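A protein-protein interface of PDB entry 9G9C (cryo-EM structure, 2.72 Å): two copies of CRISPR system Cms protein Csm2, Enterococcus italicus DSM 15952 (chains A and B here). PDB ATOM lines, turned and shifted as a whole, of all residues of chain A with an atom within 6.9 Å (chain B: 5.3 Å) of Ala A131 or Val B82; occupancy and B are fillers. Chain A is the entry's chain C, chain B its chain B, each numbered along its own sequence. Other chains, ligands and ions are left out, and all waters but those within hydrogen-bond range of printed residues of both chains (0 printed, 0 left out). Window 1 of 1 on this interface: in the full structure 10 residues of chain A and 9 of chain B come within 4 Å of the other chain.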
ATOM      1  N   LEU A  14      24.881   4.303  -7.229  1.00  0.00           N
ATOM      2  CA  LEU A  14      25.076   5.434  -6.289  1.00  0.00           C
ATOM      3  C   LEU A  14      23.987   5.289  -5.219  1.00  0.00           C
ATOM      4  O   LEU A  14      24.262   5.612  -4.049  1.00  0.00           O
ATOM      5  CB  LEU A  14      24.988   6.749  -7.056  1.00  0.00           C
ATOM      6  CG  LEU A  14      25.792   6.820  -8.359  1.00  0.00           C
ATOM      7  CD1 LEU A  14      25.628   8.168  -9.037  1.00  0.00           C
ATOM      8  CD2 LEU A  14      27.262   6.513  -8.140  1.00  0.00           C
ATOM      9  N   ASN A  15      22.785   4.851  -5.607  1.00  0.00           N
ATOM     10  CA  ASN A  15      21.769   4.535  -4.611  1.00  0.00           C
ATOM     11  C   ASN A  15      22.265   3.456  -3.659  1.00  0.00           C
ATOM     12  O   ASN A  15      22.044   3.536  -2.446  1.00  0.00           O
ATOM     13  CB  ASN A  15      20.479   4.090  -5.300  1.00  0.00           C
ATOM     14  CG  ASN A  15      20.237   4.814  -6.608  1.00  0.00           C
ATOM     15  OD1 ASN A  15      20.165   4.194  -7.669  1.00  0.00           O
ATOM     16  ND2 ASN A  15      20.112   6.134  -6.539  1.00  0.00           N
ATOM     17  N   ALA A  17      25.385   3.035  -3.012  1.00  0.00           N
ATOM     18  CA  ALA A  17      26.388   3.721  -2.204  1.00  0.00           C
ATOM     19  C   ALA A  17      25.742   4.393  -0.999  1.00  0.00           C
ATOM     20  O   ALA A  17      26.222   4.262   0.133  1.00  0.00           O
ATOM     21  CB  ALA A  17      27.144   4.740  -3.056  1.00  0.00           C
ATOM     22  N   VAL A  21      26.325   3.256   2.890  1.00  0.00           N
ATOM     23  CA  VAL A  21      26.817   4.250   3.839  1.00  0.00           C
ATOM     24  C   VAL A  21      25.868   4.377   5.025  1.00  0.00           C
ATOM     25  O   VAL A  21      26.305   4.471   6.177  1.00  0.00           O
ATOM     26  CB  VAL A  21      27.038   5.602   3.139  1.00  0.00           C
ATOM     27  CG1 VAL A  21      27.280   6.692   4.165  1.00  0.00           C
ATOM     28  CG2 VAL A  21      28.220   5.517   2.189  1.00  0.00           C
ATOM     29  N   LEU A  47      39.121   7.791   4.246  1.00  0.00           N
ATOM     30  CA  LEU A  47      38.306   7.833   3.041  1.00  0.00           C
ATOM     31  C   LEU A  47      38.911   8.770   2.006  1.00  0.00           C
ATOM     32  O   LEU A  47      38.944   8.453   0.814  1.00  0.00           O
ATOM     33  CB  LEU A  47      36.885   8.264   3.396  1.00  0.00           C
ATOM     34  CG  LEU A  47      35.769   7.750   2.494  1.00  0.00           C
ATOM     35  CD1 LEU A  47      35.700   6.240   2.561  1.00  0.00           C
ATOM     36  CD2 LEU A  47      34.454   8.361   2.914  1.00  0.00           C
ATOM     37  N   LEU A  51      40.399   8.064  -1.642  1.00  0.00           N
ATOM     38  CA  LEU A  51      39.899   8.865  -2.752  1.00  0.00           C
ATOM     39  C   LEU A  51      41.036   9.409  -3.610  1.00  0.00           C
ATOM     40  O   LEU A  51      40.918   9.448  -4.834  1.00  0.00           O
ATOM     41  CB  LEU A  51      39.025  10.002  -2.229  1.00  0.00           C
ATOM     42  CG  LEU A  51      38.239  10.766  -3.294  1.00  0.00           C
ATOM     43  CD1 LEU A  51      37.432   9.805  -4.147  1.00  0.00           C
ATOM     44  CD2 LEU A  51      37.331  11.792  -2.645  1.00  0.00           C
ATOM     45  N   LYS A 124      32.912   7.108 -10.079  1.00  0.00           N
ATOM     46  CA  LYS A 124      31.690   7.814  -9.617  1.00  0.00           C
ATOM     47  C   LYS A 124      31.143   7.100  -8.374  1.00  0.00           C
ATOM     48  O   LYS A 124      30.703   7.793  -7.439  1.00  0.00           O
ATOM     49  CB  LYS A 124      30.612   7.869 -10.704  1.00  0.00           C
ATOM     50  CG  LYS A 124      30.635   9.121 -11.565  1.00  0.00           C
ATOM     51  CD  LYS A 124      29.315   9.346 -12.292  1.00  0.00           C
ATOM     52  CE  LYS A 124      29.273  10.644 -13.032  1.00  0.00           C
ATOM     53  NZ  LYS A 124      27.968  10.861 -13.662  1.00  0.00           N
ATOM     54  N   TYR A 125      31.163   5.767  -8.375  1.00  0.00           N
ATOM     55  CA  TYR A 125      30.659   5.021  -7.225  1.00  0.00           C
ATOM     56  C   TYR A 125      31.466   5.326  -5.967  1.00  0.00           C
ATOM     57  O   TYR A 125      30.895   5.536  -4.890  1.00  0.00           O
ATOM     58  CB  TYR A 125      30.676   3.524  -7.525  1.00  0.00           C
ATOM     59  CG  TYR A 125      30.410   2.652  -6.320  1.00  0.00           C
ATOM     60  CD1 TYR A 125      29.137   2.551  -5.780  1.00  0.00           C
ATOM     61  CD2 TYR A 125      31.432   1.925  -5.728  1.00  0.00           C
ATOM     62  CE1 TYR A 125      28.889   1.753  -4.681  1.00  0.00           C
ATOM     63  CE2 TYR A 125      31.194   1.125  -4.629  1.00  0.00           C
ATOM     64  CZ  TYR A 125      29.921   1.043  -4.110  1.00  0.00           C
ATOM     65  OH  TYR A 125      29.681   0.246  -3.016  1.00  0.00           O
ATOM     66  N   PHE A 126      32.795   5.354  -6.084  1.00  0.00           N
ATOM     67  CA  PHE A 126      33.625   5.712  -4.934  1.00  0.00           C
ATOM     68  C   PHE A 126      33.371   7.156  -4.508  1.00  0.00           C
ATOM     69  O   PHE A 126      33.346   7.473  -3.310  1.00  0.00           O
ATOM     70  CB  PHE A 126      35.100   5.496  -5.269  1.00  0.00           C
ATOM     71  CG  PHE A 126      35.949   5.158  -4.079  1.00  0.00           C
ATOM     72  CD1 PHE A 126      35.994   3.864  -3.590  1.00  0.00           C
ATOM     73  CD2 PHE A 126      36.708   6.131  -3.450  1.00  0.00           C
ATOM     74  CE1 PHE A 126      36.773   3.546  -2.497  1.00  0.00           C
ATOM     75  CE2 PHE A 126      37.489   5.818  -2.356  1.00  0.00           C
ATOM     76  CZ  PHE A 126      37.521   4.524  -1.879  1.00  0.00           C
ATOM     77  N   GLU A 127      33.175   8.042  -5.486  1.00  0.00           N
ATOM     78  CA  GLU A 127      32.842   9.431  -5.199  1.00  0.00           C
ATOM     79  C   GLU A 127      31.529   9.535  -4.436  1.00  0.00           C
ATOM     80  O   GLU A 127      31.410  10.326  -3.495  1.00  0.00           O
ATOM     81  CB  GLU A 127      32.765  10.207  -6.512  1.00  0.00           C
ATOM     82  CG  GLU A 127      32.555  11.690  -6.371  1.00  0.00           C
ATOM     83  CD  GLU A 127      32.611  12.396  -7.708  1.00  0.00           C
ATOM     84  OE1 GLU A 127      32.729  11.699  -8.737  1.00  0.00           O
ATOM     85  OE2 GLU A 127      32.535  13.640  -7.736  1.00  0.00           O
ATOM     86  N   ALA A 128      30.530   8.744  -4.832  1.00  0.00           N
ATOM     87  CA  ALA A 128      29.257   8.731  -4.121  1.00  0.00           C
ATOM     88  C   ALA A 128      29.419   8.172  -2.715  1.00  0.00           C
ATOM     89  O   ALA A 128      28.757   8.634  -1.782  1.00  0.00           O
ATOM     90  CB  ALA A 128      28.225   7.922  -4.903  1.00  0.00           C
ATOM     91  N   LEU A 129      30.281   7.167  -2.548  1.00  0.00           N
ATOM     92  CA  LEU A 129      30.582   6.673  -1.206  1.00  0.00           C
ATOM     93  C   LEU A 129      31.110   7.796  -0.323  1.00  0.00           C
ATOM     94  O   LEU A 129      30.631   8.000   0.800  1.00  0.00           O
ATOM     95  CB  LEU A 129      31.600   5.533  -1.279  1.00  0.00           C
ATOM     96  CG  LEU A 129      31.151   4.203  -1.880  1.00  0.00           C
ATOM     97  CD1 LEU A 129      32.330   3.253  -1.975  1.00  0.00           C
ATOM     98  CD2 LEU A 129      30.038   3.596  -1.052  1.00  0.00           C
ATOM     99  N   VAL A 130      32.088   8.549  -0.831  1.00  0.00           N
ATOM    100  CA  VAL A 130      32.652   9.656  -0.059  1.00  0.00           C
ATOM    101  C   VAL A 130      31.589  10.714   0.221  1.00  0.00           C
ATOM    102  O   VAL A 130      31.490  11.240   1.339  1.00  0.00           O
ATOM    103  CB  VAL A 130      33.867  10.254  -0.794  1.00  0.00           C
ATOM    104  CG1 VAL A 130      34.421  11.443  -0.025  1.00  0.00           C
ATOM    105  CG2 VAL A 130      34.939   9.198  -0.992  1.00  0.00           C
ATOM    106  N   ALA A 131      30.780  11.042  -0.788  1.00  0.00           N
ATOM    107  CA  ALA A 131      29.775  12.089  -0.638  1.00  0.00           C
ATOM    108  C   ALA A 131      28.722  11.712   0.395  1.00  0.00           C
ATOM    109  O   ALA A 131      28.323  12.545   1.216  1.00  0.00           O
ATOM    110  CB  ALA A 131      29.119  12.377  -1.987  1.00  0.00           C
ATOM    111  N   TYR A 132      28.256  10.464   0.369  1.00  0.00           N
ATOM    112  CA  TYR A 132      27.245  10.032   1.325  1.00  0.00           C
ATOM    113  C   TYR A 132      27.826   9.853   2.720  1.00  0.00           C
ATOM    114  O   TYR A 132      27.111  10.033   3.710  1.00  0.00           O
ATOM    115  CB  TYR A 132      26.581   8.746   0.839  1.00  0.00           C
ATOM    116  CG  TYR A 132      25.634   8.967  -0.320  1.00  0.00           C
ATOM    117  CD1 TYR A 132      24.621   9.913  -0.240  1.00  0.00           C
ATOM    118  CD2 TYR A 132      25.760   8.243  -1.497  1.00  0.00           C
ATOM    119  CE1 TYR A 132      23.756  10.123  -1.295  1.00  0.00           C
ATOM    120  CE2 TYR A 132      24.899   8.448  -2.558  1.00  0.00           C
ATOM    121  CZ  TYR A 132      23.900   9.388  -2.451  1.00  0.00           C
ATOM    122  OH  TYR A 132      23.040   9.596  -3.504  1.00  0.00           O
ATOM    123  N   ALA A 133      29.109   9.498   2.828  1.00  0.00           N
ATOM    124  CA  ALA A 133      29.749   9.507   4.139  1.00  0.00           C
ATOM    125  C   ALA A 133      29.820  10.921   4.701  1.00  0.00           C
ATOM    126  O   ALA A 133      29.614  11.131   5.901  1.00  0.00           O
ATOM    127  CB  ALA A 133      31.142   8.891   4.049  1.00  0.00           C
ATOM    128  N   LYS A 134      30.120  11.903   3.846  1.00  0.00           N
ATOM    129  CA  LYS A 134      30.086  13.298   4.280  1.00  0.00           C
ATOM    130  C   LYS A 134      28.678  13.716   4.686  1.00  0.00           C
ATOM    131  O   LYS A 134      28.495  14.445   5.668  1.00  0.00           O
ATOM    132  CB  LYS A 134      30.608  14.207   3.168  1.00  0.00           C
ATOM    133  CG  LYS A 134      31.877  14.966   3.518  1.00  0.00           C
ATOM    134  CD  LYS A 134      31.644  15.943   4.655  1.00  0.00           C
ATOM    135  CE  LYS A 134      32.912  16.711   4.988  1.00  0.00           C
ATOM    136  NZ  LYS A 134      32.691  17.705   6.072  1.00  0.00           N
ATOM    137  N   PHE A 135      27.671  13.272   3.931  1.00  0.00           N
ATOM    138  CA  PHE A 135      26.293  13.665   4.205  1.00  0.00           C
ATOM    139  C   PHE A 135      25.814  13.136   5.551  1.00  0.00           C
ATOM    140  O   PHE A 135      25.147  13.853   6.307  1.00  0.00           O
ATOM    141  CB  PHE A 135      25.383  13.171   3.080  1.00  0.00           C
ATOM    142  CG  PHE A 135      23.930  13.477   3.292  1.00  0.00           C
ATOM    143  CD1 PHE A 135      23.438  14.752   3.072  1.00  0.00           C
ATOM    144  CD2 PHE A 135      23.054  12.485   3.696  1.00  0.00           C
ATOM    145  CE1 PHE A 135      22.101  15.034   3.262  1.00  0.00           C
ATOM    146  CE2 PHE A 135      21.715  12.762   3.887  1.00  0.00           C
ATOM    147  CZ  PHE A 135      21.238  14.037   3.669  1.00  0.00           C
ATOM    148  N   TYR A 136      26.145  11.889   5.872  1.00  0.00           N
ATOM    149  CA  TYR A 136      25.676  11.255   7.097  1.00  0.00           C
ATOM    150  C   TYR A 136      26.575  11.532   8.294  1.00  0.00           C
ATOM    151  O   TYR A 136      26.304  11.019   9.385  1.00  0.00           O
ATOM    152  CB  TYR A 136      25.547   9.742   6.891  1.00  0.00           C
ATOM    153  CG  TYR A 136      24.318   9.335   6.110  1.00  0.00           C
ATOM    154  CD1 TYR A 136      23.082   9.229   6.731  1.00  0.00           C
ATOM    155  CD2 TYR A 136      24.394   9.054   4.754  1.00  0.00           C
ATOM    156  CE1 TYR A 136      21.955   8.856   6.022  1.00  0.00           C
ATOM    157  CE2 TYR A 136      23.274   8.681   4.037  1.00  0.00           C
ATOM    158  CZ  TYR A 136      22.058   8.584   4.676  1.00  0.00           C
ATOM    159  OH  TYR A 136      20.939   8.211   3.968  1.00  0.00           O
ATOM    160  N   GLU B  78      21.491  11.071 -11.336  1.00  0.00           N
ATOM    161  CA  GLU B  78      21.867  10.326 -10.107  1.00  0.00           C
ATOM    162  C   GLU B  78      23.101  10.995  -9.491  1.00  0.00           C
ATOM    163  O   GLU B  78      23.141  11.144  -8.253  1.00  0.00           O
ATOM    164  CB  GLU B  78      22.120   8.864 -10.464  1.00  0.00           C
ATOM    165  CG  GLU B  78      20.891   8.165 -11.040  1.00  0.00           C
ATOM    166  CD  GLU B  78      19.967   7.557 -10.002  1.00  0.00           C
ATOM    167  OE1 GLU B  78      20.310   7.600  -8.803  1.00  0.00           O
ATOM    168  OE2 GLU B  78      18.901   7.041 -10.396  1.00  0.00           O
ATOM    169  N   TYR B  79      24.048  11.406 -10.333  1.00  0.00           N
ATOM    170  CA  TYR B  79      25.277  12.090  -9.858  1.00  0.00           C
ATOM    171  C   TYR B  79      24.874  13.392  -9.189  1.00  0.00           C
ATOM    172  O   TYR B  79      25.484  13.775  -8.177  1.00  0.00           O
ATOM    173  CB  TYR B  79      26.207  12.353 -11.042  1.00  0.00           C
ATOM    174  CG  TYR B  79      27.548  12.967 -10.667  1.00  0.00           C
ATOM    175  CD1 TYR B  79      28.233  12.556  -9.530  1.00  0.00           C
ATOM    176  CD2 TYR B  79      28.111  13.975 -11.436  1.00  0.00           C
ATOM    177  CE1 TYR B  79      29.450  13.118  -9.182  1.00  0.00           C
ATOM    178  CE2 TYR B  79      29.325  14.547 -11.097  1.00  0.00           C
ATOM    179  CZ  TYR B  79      29.996  14.116  -9.968  1.00  0.00           C
ATOM    180  OH  TYR B  79      31.191  14.685  -9.636  1.00  0.00           O
ATOM    181  N   LEU B  80      23.869  14.068  -9.748  1.00  0.00           N
ATOM    182  CA  LEU B  80      23.418  15.369  -9.195  1.00  0.00           C
ATOM    183  C   LEU B  80      22.976  15.170  -7.739  1.00  0.00           C
ATOM    184  O   LEU B  80      23.367  15.988  -6.885  1.00  0.00           O
ATOM    185  CB  LEU B  80      22.283  15.896 -10.069  1.00  0.00           C
ATOM    186  CG  LEU B  80      21.690  17.251  -9.681  1.00  0.00           C
ATOM    187  CD1 LEU B  80      22.743  18.338  -9.784  1.00  0.00           C
ATOM    188  CD2 LEU B  80      20.518  17.549 -10.596  1.00  0.00           C
ATOM    189  N   LYS B  81      22.202  14.116  -7.475  1.00  0.00           N
ATOM    190  CA  LYS B  81      21.746  13.830  -6.091  1.00  0.00           C
ATOM    191  C   LYS B  81      22.966  13.517  -5.212  1.00  0.00           C
ATOM    192  O   LYS B  81      22.954  13.907  -4.029  1.00  0.00           O
ATOM    193  CB  LYS B  81      20.745  12.675  -6.119  1.00  0.00           C
ATOM    194  CG  LYS B  81      19.612  12.891  -7.103  1.00  0.00           C
ATOM    195  CD  LYS B  81      18.684  11.689  -7.178  1.00  0.00           C
ATOM    196  CE  LYS B  81      19.460  10.415  -7.223  1.00  0.00           C
ATOM    197  NZ  LYS B  81      18.581   9.244  -7.254  1.00  0.00           N
ATOM    198  N   VAL B  82      23.976  12.848  -5.771  1.00  0.00           N
ATOM    199  CA  VAL B  82      25.226  12.576  -5.001  1.00  0.00           C
ATOM    200  C   VAL B  82      25.932  13.908  -4.713  1.00  0.00           C
ATOM    201  O   VAL B  82      26.412  14.089  -3.577  1.00  0.00           O
ATOM    202  CB  VAL B  82      26.125  11.625  -5.810  1.00  0.00           C
ATOM    203  CG1 VAL B  82      27.581  11.669  -5.368  1.00  0.00           C
ATOM    204  CG2 VAL B  82      25.581  10.204  -5.822  1.00  0.00           C
ATOM    205  N   LYS B  83      25.962  14.810  -5.694  1.00  0.00           N
ATOM    206  CA  LYS B  83      26.578  16.145  -5.487  1.00  0.00           C
ATOM    207  C   LYS B  83      25.717  16.931  -4.493  1.00  0.00           C
ATOM    208  O   LYS B  83      26.293  17.588  -3.609  1.00  0.00           O
ATOM    209  CB  LYS B  83      26.705  16.882  -6.821  1.00  0.00           C
ATOM    210  CG  LYS B  83      27.735  16.282  -7.761  1.00  0.00           C
ATOM    211  CD  LYS B  83      29.121  16.158  -7.137  1.00  0.00           C
ATOM    212  CE  LYS B  83      29.928  17.417  -7.183  1.00  0.00           C
ATOM    213  NZ  LYS B  83      29.592  18.361  -6.115  1.00  0.00           N
ATOM    214  N   PHE B  84      24.391  16.863  -4.637  1.00  0.00           N
ATOM    215  CA  PHE B  84      23.497  17.525  -3.649  1.00  0.00           C
ATOM    216  C   PHE B  84      23.878  17.033  -2.260  1.00  0.00           C
ATOM    217  O   PHE B  84      24.143  17.872  -1.377  1.00  0.00           O
ATOM    218  CB  PHE B  84      22.018  17.256  -3.933  1.00  0.00           C
ATOM    219  CG  PHE B  84      21.444  18.124  -5.042  1.00  0.00           C
ATOM    220  CD1 PHE B  84      21.990  19.371  -5.320  1.00  0.00           C
ATOM    221  CD2 PHE B  84      20.356  17.697  -5.792  1.00  0.00           C
ATOM    222  CE1 PHE B  84      21.468  20.165  -6.326  1.00  0.00           C
ATOM    223  CE2 PHE B  84      19.837  18.497  -6.794  1.00  0.00           C
ATOM    224  CZ  PHE B  84      20.394  19.726  -7.060  1.00  0.00           C
ATOM    225  N   ALA B  85      23.916  15.709  -2.076  1.00  0.00           N
ATOM    226  CA  ALA B  85      24.249  15.158  -0.765  1.00  0.00           C
ATOM    227  C   ALA B  85      25.615  15.639  -0.290  1.00  0.00           C
ATOM    228  O   ALA B  85      25.786  15.979   0.887  1.00  0.00           O
ATOM    229  CB  ALA B  85      24.208  13.631  -0.812  1.00  0.00           C
ATOM    230  N   TYR B  86      26.598  15.677  -1.192  1.00  0.00           N
ATOM    231  CA  TYR B  86      27.939  16.113  -0.812  1.00  0.00           C
ATOM    232  C   TYR B  86      27.939  17.563  -0.344  1.00  0.00           C
ATOM    233  O   TYR B  86      28.528  17.894   0.692  1.00  0.00           O
ATOM    234  CB  TYR B  86      28.899  15.931  -1.987  1.00  0.00           C
ATOM    235  CG  TYR B  86      30.302  16.421  -1.715  1.00  0.00           C
ATOM    236  CD1 TYR B  86      31.127  15.757  -0.818  1.00  0.00           C
ATOM    237  CD2 TYR B  86      30.805  17.542  -2.359  1.00  0.00           C
ATOM    238  CE1 TYR B  86      32.410  16.199  -0.567  1.00  0.00           C
ATOM    239  CE2 TYR B  86      32.088  17.991  -2.115  1.00  0.00           C
ATOM    240  CZ  TYR B  86      32.885  17.316  -1.219  1.00  0.00           C
ATOM    241  OH  TYR B  86      34.163  17.758  -0.972  1.00  0.00           O
ATOM    242  N   GLU B  87      27.275  18.443  -1.094  1.00  0.00           N
ATOM    243  CA  GLU B  87      27.238  19.852  -0.718  1.00  0.00           C
ATOM    244  C   GLU B  87      26.428  20.066   0.554  1.00  0.00           C
ATOM    245  O   GLU B  87      26.771  20.924   1.374  1.00  0.00           O
ATOM    246  CB  GLU B  87      26.678  20.695  -1.864  1.00  0.00           C
ATOM    247  CG  GLU B  87      27.401  20.528  -3.193  1.00  0.00           C
ATOM    248  CD  GLU B  87      28.875  20.871  -3.117  1.00  0.00           C
ATOM    249  OE1 GLU B  87      29.256  21.702  -2.266  1.00  0.00           O
ATOM    250  OE2 GLU B  87      29.656  20.311  -3.914  1.00  0.00           O
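Glu B78 touches Leu A14 (C to CD1, 3.8 Å).
Leu A14 touches Tyr B79.
CB of Leu A14 touches CG2 of Val B82, 3.7 Å away.
Asn A15 touches Lys B81.
Tyr B79 touches Lys A124.
Val B82 touches Ala A128.
CB of Ala A131 touches O of Val B82, 3.6 Å away.
Val B82 touches Tyr A132.
Tyr A132 touches Ala B85.
CD1 of Phe A135 touches O of Ala B85 (3.4 Å).
OE2 of Glu A127 sits at hydrogen-bond distance from OH of Tyr B79 (2.6 Å).
OE1 of Glu B78 is in hydrogen-bond range of ND2 of Asn A15 (2.7 Å).
Printed residues of chain B within 4 Å of Phe A135: Ala B85.
Printed residues of chain A within 4 Å of Tyr B79: Leu A14, Lys A124 and Glu A127.
Of the printed residues of chain A, Val B82 touches Leu A14, Ala A128, Ala A131 and Tyr A132.
Of the printed residues of chain A, Tyr B86 touches Ala A131 (3.6 Å).
The nearest printed residue of chain A that does not touch Lys B81 is Tyr A132 (4.3 Å).
No position is printed for both chains.
Of the 19 printed residues of chain A, 8 touch a printed residue of chain B.
Printed residues of chain A that touch a printed residue of chain B: Leu A14, Asn A15, Lys A124, Glu A127, Ala A128, Ala A131, Tyr A132 and Phe A135.
Hydrophobic or aromatic side chains of chain A within 4 Å of the printed part of chain B: Leu A14, Ala A128, Ala A131, Tyr A132 and Phe A135.
Of the 10 printed residues of chain B, 6 touch a printed residue of chain A.
Among the printed residues, 13 pairs touch across the chains.
The side-chain carboxylate of Glu B78 lies within salt-bridge range of the side-chain amino group of Lys B81 (2.8 Å).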
